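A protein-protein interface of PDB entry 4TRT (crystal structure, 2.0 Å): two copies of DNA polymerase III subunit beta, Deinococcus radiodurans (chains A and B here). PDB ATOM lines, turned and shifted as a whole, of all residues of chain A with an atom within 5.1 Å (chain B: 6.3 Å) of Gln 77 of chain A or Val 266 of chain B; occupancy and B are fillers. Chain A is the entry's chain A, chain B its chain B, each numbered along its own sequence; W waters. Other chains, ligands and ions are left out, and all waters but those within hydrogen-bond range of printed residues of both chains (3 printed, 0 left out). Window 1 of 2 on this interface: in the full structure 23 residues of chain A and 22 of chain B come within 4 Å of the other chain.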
ATOM      1  N   GLU A  19      11.206  21.978  -3.266  1.00  0.00           N
ATOM      2  CA  GLU A  19      10.386  23.061  -2.742  1.00  0.00           C
ATOM      3  C   GLU A  19      10.326  24.273  -3.677  1.00  0.00           C
ATOM      4  O   GLU A  19       9.363  25.034  -3.628  1.00  0.00           O
ATOM      5  CB  GLU A  19      10.820  23.470  -1.329  1.00  0.00           C
ATOM      6  CG  GLU A  19      11.943  24.476  -1.244  1.00  0.00           C
ATOM      7  CD  GLU A  19      12.234  24.914   0.184  1.00  0.00           C
ATOM      8  OE1 GLU A  19      13.414  25.134   0.496  1.00  0.00           O
ATOM      9  OE2 GLU A  19      11.300  25.052   0.998  1.00  0.00           O
ATOM     10  N   ALA A  72       5.258  19.847   1.288  1.00  0.00           N
ATOM     11  CA  ALA A  72       6.636  19.960   0.848  1.00  0.00           C
ATOM     12  C   ALA A  72       7.412  21.070   1.554  1.00  0.00           C
ATOM     13  O   ALA A  72       8.553  20.852   1.964  1.00  0.00           O
ATOM     14  CB  ALA A  72       6.699  20.151  -0.664  1.00  0.00           C
ATOM     15  N   HIS A  73       6.815  22.251   1.702  1.00  0.00           N
ATOM     16  CA  HIS A  73       7.565  23.394   2.246  1.00  0.00           C
ATOM     17  C   HIS A  73       7.773  23.294   3.727  1.00  0.00           C
ATOM     18  O   HIS A  73       8.848  23.633   4.242  1.00  0.00           O
ATOM     19  CB  HIS A  73       6.915  24.707   1.852  1.00  0.00           C
ATOM     20  CG  HIS A  73       6.959  24.952   0.376  1.00  0.00           C
ATOM     21  ND1 HIS A  73       6.105  24.339  -0.476  1.00  0.00           N
ATOM     22  CD2 HIS A  73       7.808  25.732  -0.406  1.00  0.00           C
ATOM     23  CE1 HIS A  73       6.389  24.700  -1.730  1.00  0.00           C
ATOM     24  NE2 HIS A  73       7.427  25.555  -1.699  1.00  0.00           N
ATOM     25  N   LEU A  74       6.758  22.809   4.427  1.00  0.00           N
ATOM     26  CA  LEU A  74       6.871  22.567   5.855  1.00  0.00           C
ATOM     27  C   LEU A  74       7.958  21.529   6.158  1.00  0.00           C
ATOM     28  O   LEU A  74       8.759  21.735   7.046  1.00  0.00           O
ATOM     29  CB  LEU A  74       5.522  22.125   6.438  1.00  0.00           C
ATOM     30  CG  LEU A  74       5.511  21.772   7.926  1.00  0.00           C
ATOM     31  CD1 LEU A  74       6.078  22.936   8.734  1.00  0.00           C
ATOM     32  CD2 LEU A  74       4.089  21.471   8.375  1.00  0.00           C
ATOM     33  N   PHE A  75       7.976  20.425   5.413  1.00  0.00           N
ATOM     34  CA  PHE A  75       8.964  19.370   5.615  1.00  0.00           C
ATOM     35  C   PHE A  75      10.384  19.879   5.353  1.00  0.00           C
ATOM     36  O   PHE A  75      11.290  19.595   6.119  1.00  0.00           O
ATOM     37  CB  PHE A  75       8.635  18.164   4.736  1.00  0.00           C
ATOM     38  CG  PHE A  75       9.567  16.988   4.899  1.00  0.00           C
ATOM     39  CD1 PHE A  75       9.967  16.550   6.155  1.00  0.00           C
ATOM     40  CD2 PHE A  75       9.986  16.268   3.797  1.00  0.00           C
ATOM     41  CE1 PHE A  75      10.813  15.463   6.296  1.00  0.00           C
ATOM     42  CE2 PHE A  75      10.819  15.163   3.935  1.00  0.00           C
ATOM     43  CZ  PHE A  75      11.241  14.770   5.196  1.00  0.00           C
ATOM     44  N   ALA A  76      10.550  20.662   4.290  1.00  0.00           N
ATOM     45  CA  ALA A  76      11.837  21.249   3.950  1.00  0.00           C
ATOM     46  C   ALA A  76      12.315  22.200   5.044  1.00  0.00           C
ATOM     47  O   ALA A  76      13.487  22.225   5.400  1.00  0.00           O
ATOM     48  CB  ALA A  76      11.741  21.988   2.617  1.00  0.00           C
ATOM     49  N   GLN A  77      11.384  22.975   5.581  1.00  0.00           N
ATOM     50  CA  GLN A  77      11.698  23.934   6.630  1.00  0.00           C
ATOM     51  C   GLN A  77      12.123  23.236   7.918  1.00  0.00           C
ATOM     52  O   GLN A  77      13.064  23.661   8.591  1.00  0.00           O
ATOM     53  CB  GLN A  77      10.486  24.848   6.866  1.00  0.00           C
ATOM     54  CG  GLN A  77      10.641  25.844   8.012  1.00  0.00           C
ATOM     55  CD  GLN A  77       9.415  26.732   8.155  1.00  0.00           C
ATOM     56  OE1 GLN A  77       8.331  26.383   7.692  1.00  0.00           O
ATOM     57  NE2 GLN A  77       9.583  27.881   8.788  1.00  0.00           N
ATOM     58  N   ILE A  78      11.401  22.184   8.289  1.00  0.00           N
ATOM     59  CA  ILE A  78      11.723  21.423   9.500  1.00  0.00           C
ATOM     60  C   ILE A  78      13.131  20.815   9.381  1.00  0.00           C
ATOM     61  O   ILE A  78      13.943  20.908  10.308  1.00  0.00           O
ATOM     62  CB  ILE A  78      10.658  20.340   9.742  1.00  0.00           C
ATOM     63  CG1 ILE A  78       9.371  20.973  10.281  1.00  0.00           C
ATOM     64  CG2 ILE A  78      11.172  19.252  10.675  1.00  0.00           C
ATOM     65  CD1 ILE A  78       8.202  19.987  10.311  1.00  0.00           C
ATOM     66  N   VAL A  79      13.436  20.248   8.221  1.00  0.00           N
ATOM     67  CA  VAL A  79      14.740  19.595   8.027  1.00  0.00           C
ATOM     68  C   VAL A  79      15.865  20.629   8.046  1.00  0.00           C
ATOM     69  O   VAL A  79      16.870  20.436   8.711  1.00  0.00           O
ATOM     70  CB  VAL A  79      14.774  18.754   6.735  1.00  0.00           C
ATOM     71  CG1 VAL A  79      16.182  18.186   6.466  1.00  0.00           C
ATOM     72  CG2 VAL A  79      13.768  17.623   6.821  1.00  0.00           C
ATOM     73  N   ARG A  80      15.662  21.749   7.364  1.00  0.00           N
ATOM     74  CA  ARG A  80      16.627  22.835   7.376  1.00  0.00           C
ATOM     75  C   ARG A  80      16.962  23.323   8.780  1.00  0.00           C
ATOM     76  O   ARG A  80      18.121  23.580   9.065  1.00  0.00           O
ATOM     77  CB  ARG A  80      16.074  23.968   6.535  1.00  0.00           C
ATOM     78  CG  ARG A  80      16.841  25.282   6.529  1.00  0.00           C
ATOM     79  CD  ARG A  80      16.110  26.314   5.683  1.00  0.00           C
ATOM     80  NE  ARG A  80      15.586  25.717   4.465  1.00  0.00           N
ATOM     81  CZ  ARG A  80      14.324  25.779   4.034  1.00  0.00           C
ATOM     82  NH1 ARG A  80      13.382  26.449   4.685  1.00  0.00           N
ATOM     83  NH2 ARG A  80      14.007  25.175   2.900  1.00  0.00           N
ATOM     84  N   ASN A  81      15.953  23.416   9.647  1.00  0.00           N
ATOM     85  CA  ASN A  81      16.125  23.939  10.995  1.00  0.00           C
ATOM     86  C   ASN A  81      16.726  22.943  11.987  1.00  0.00           C
ATOM     87  O   ASN A  81      17.055  23.316  13.109  1.00  0.00           O
ATOM     88  CB  ASN A  81      14.772  24.432  11.547  1.00  0.00           C
ATOM     89  CG  ASN A  81      14.268  25.685  10.852  1.00  0.00           C
ATOM     90  OD1 ASN A  81      15.041  26.420  10.227  1.00  0.00           O
ATOM     91  ND2 ASN A  81      12.960  25.953  10.971  1.00  0.00           N
ATOM     92  N   VAL B 261      13.798  27.506  20.173  1.00  0.00           N
ATOM     93  CA  VAL B 261      12.484  28.152  20.156  1.00  0.00           C
ATOM     94  C   VAL B 261      12.053  28.366  18.697  1.00  0.00           C
ATOM     95  O   VAL B 261      10.919  28.066  18.321  1.00  0.00           O
ATOM     96  CB  VAL B 261      12.495  29.491  20.939  1.00  0.00           C
ATOM     97  CG1 VAL B 261      11.223  30.296  20.686  1.00  0.00           C
ATOM     98  CG2 VAL B 261      12.680  29.235  22.420  1.00  0.00           C
ATOM     99  N   ASN B 262      12.989  28.846  17.879  1.00  0.00           N
ATOM    100  CA  ASN B 262      12.743  29.062  16.479  1.00  0.00           C
ATOM    101  C   ASN B 262      12.251  27.797  15.764  1.00  0.00           C
ATOM    102  O   ASN B 262      11.208  27.823  15.111  1.00  0.00           O
ATOM    103  CB  ASN B 262      13.995  29.579  15.768  1.00  0.00           C
ATOM    104  CG  ASN B 262      13.737  29.862  14.308  1.00  0.00           C
ATOM    105  OD1 ASN B 262      12.950  30.757  13.979  1.00  0.00           O
ATOM    106  ND2 ASN B 262      14.355  29.068  13.416  1.00  0.00           N
ATOM    107  N   ARG B 263      12.980  26.701  15.906  1.00  0.00           N
ATOM    108  CA  ARG B 263      12.613  25.490  15.198  1.00  0.00           C
ATOM    109  C   ARG B 263      11.283  24.890  15.670  1.00  0.00           C
ATOM    110  O   ARG B 263      10.478  24.479  14.839  1.00  0.00           O
ATOM    111  CB  ARG B 263      13.754  24.454  15.204  1.00  0.00           C
ATOM    112  CG  ARG B 263      14.061  23.773  16.518  1.00  0.00           C
ATOM    113  CD  ARG B 263      15.072  22.643  16.311  1.00  0.00           C
ATOM    114  NE  ARG B 263      16.352  23.150  15.830  1.00  0.00           N
ATOM    115  CZ  ARG B 263      17.375  23.510  16.607  1.00  0.00           C
ATOM    116  NH1 ARG B 263      17.321  23.394  17.931  1.00  0.00           N
ATOM    117  NH2 ARG B 263      18.478  23.982  16.051  1.00  0.00           N
ATOM    118  N   VAL B 264      11.044  24.867  16.982  1.00  0.00           N
ATOM    119  CA  VAL B 264       9.810  24.292  17.531  1.00  0.00           C
ATOM    120  C   VAL B 264       8.573  25.136  17.152  1.00  0.00           C
ATOM    121  O   VAL B 264       7.515  24.592  16.855  1.00  0.00           O
ATOM    122  CB  VAL B 264       9.925  24.085  19.061  1.00  0.00           C
ATOM    123  CG1 VAL B 264       8.565  23.850  19.721  1.00  0.00           C
ATOM    124  CG2 VAL B 264      10.873  22.927  19.362  1.00  0.00           C
ATOM    125  N   ALA B 265       8.735  26.460  17.117  1.00  0.00           N
ATOM    126  CA  ALA B 265       7.627  27.386  16.872  1.00  0.00           C
ATOM    127  C   ALA B 265       7.030  27.222  15.485  1.00  0.00           C
ATOM    128  O   ALA B 265       5.891  27.625  15.249  1.00  0.00           O
ATOM    129  CB  ALA B 265       8.083  28.832  17.087  1.00  0.00           C
ATOM    130  N   VAL B 266       7.769  26.604  14.563  1.00  0.00           N
ATOM    131  CA  VAL B 266       7.252  26.392  13.225  1.00  0.00           C
ATOM    132  C   VAL B 266       5.957  25.582  13.242  1.00  0.00           C
ATOM    133  O   VAL B 266       5.136  25.766  12.366  1.00  0.00           O
ATOM    134  CB  VAL B 266       8.289  25.698  12.304  1.00  0.00           C
ATOM    135  CG1 VAL B 266       7.641  25.257  11.007  1.00  0.00           C
ATOM    136  CG2 VAL B 266       9.483  26.620  12.030  1.00  0.00           C
ATOM    137  N   LEU B 267       5.773  24.691  14.218  1.00  0.00           N
ATOM    138  CA  LEU B 267       4.550  23.871  14.277  1.00  0.00           C
ATOM    139  C   LEU B 267       3.414  24.450  15.153  1.00  0.00           C
ATOM    140  O   LEU B 267       2.374  23.816  15.297  1.00  0.00           O
ATOM    141  CB  LEU B 267       4.878  22.419  14.671  1.00  0.00           C
ATOM    142  CG  LEU B 267       5.549  21.616  13.546  1.00  0.00           C
ATOM    143  CD1 LEU B 267       5.894  20.221  14.004  1.00  0.00           C
ATOM    144  CD2 LEU B 267       4.653  21.529  12.316  1.00  0.00           C
ATOM    145  N   ALA B 268       3.618  25.637  15.727  1.00  0.00           N
ATOM    146  CA  ALA B 268       2.527  26.350  16.442  1.00  0.00           C
ATOM    147  C   ALA B 268       1.458  26.749  15.465  1.00  0.00           C
ATOM    148  O   ALA B 268       1.743  26.977  14.292  1.00  0.00           O
ATOM    149  CB  ALA B 268       3.031  27.594  17.133  1.00  0.00           C
ATOM    150  N   ASP B 269       0.233  26.884  15.951  1.00  0.00           N
ATOM    151  CA  ASP B 269      -0.857  27.261  15.064  1.00  0.00           C
ATOM    152  C   ASP B 269      -0.660  28.677  14.534  1.00  0.00           C
ATOM    153  O   ASP B 269      -0.179  29.556  15.255  1.00  0.00           O
ATOM    154  CB  ASP B 269      -2.228  27.090  15.736  1.00  0.00           C
ATOM    155  CG  ASP B 269      -2.921  25.782  15.335  1.00  0.00           C
ATOM    156  OD1 ASP B 269      -2.674  25.275  14.210  1.00  0.00           O
ATOM    157  OD2 ASP B 269      -3.726  25.263  16.139  1.00  0.00           O
ATOM    158  N   ALA B 289       5.551  22.651  20.740  1.00  0.00           N
ATOM    159  CA  ALA B 289       4.487  23.346  20.031  1.00  0.00           C
ATOM    160  C   ALA B 289       3.692  22.304  19.258  1.00  0.00           C
ATOM    161  O   ALA B 289       4.192  21.213  18.952  1.00  0.00           O
ATOM    162  CB  ALA B 289       5.029  24.407  19.085  1.00  0.00           C
HETATM  163  O   HOH W   1      14.539  29.334  10.589  1.00  0.00           O
HETATM  164  O   HOH W   2      11.534  23.863  12.385  1.00  0.00           O
HETATM  165  O   HOH W   3      19.672  24.629  13.782  1.00  0.00           O
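The backbone carbonyl oxygen (O) of Gln 77 of chain A lies close to the side-chain amide nitrogen (ND2) of Asn 81 of chain A (3.3 Å).
Water W3 bridges the guanidinium group (NH2) of Arg 263 of chain B and the backbone carbonyl oxygen (O) of Asn 81 of chain A.
Water W2 bridges the backbone carbonyl oxygen (O) of Arg 263 of chain B (2.7 Å) and the side-chain amide nitrogen (ND2) of Asn 81 of chain A (2.9 Å).
Water W1 bridges the side-chain amide nitrogen of Asn 262 of chain B (2.8 Å) and the side-chain amide oxygen of Asn 81 of chain A (3.0 Å).
Among the printed residues, pairs that only touch across the chains: Gln 77 of chain A with Val 266 of chain B (3.5 Å), Leu 74 of chain A with Val 266 of chain B (3.6 Å), Asn 81 of chain A with Val 266 of chain B (3.7 Å) and Leu 74 of chain A with Leu 267 of chain B (3.98 Å).
Printed residues of chain B within 4 Å of Gln 77 of chain A: Val 266.
Of chain A, only Leu 74, Gln 77 and Asn 81 come within 4 Å of Val 266 of chain B.
Of the printed residues of chain A, Leu 267 of chain B touches Leu 74 (3.98 Å).
Of the printed residues of chain B, Leu 74 of chain A touches Val 266 and Leu 267.
Ala 72 of chain A touches none of the printed residues of chain B.
The nearest printed residue of chain B that does not touch Gln 77 of chain A is Asn 262 of chain B (6.5 Å).
The nearest residue of chain A that does not touch Val 266 of chain B is Ile 78 of chain A (4.7 Å).
The guanidinium group (NE) of Arg 263 of chain B lies within hydrogen-bond range of the backbone carbonyl oxygen (O) of Asn 81 of chain A (2.8 Å).
No position is printed for both chains.
Hydrophobic or aromatic side chains of chain A within 4 Å of the printed part of chain B: Leu 74.
Among the printed residues, 5 pairs touch across the chains.
Among the printed residues, no Asp or Glu carboxylate lies within 4 Å of a Lys or Arg side-chain nitrogen of the other chain.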
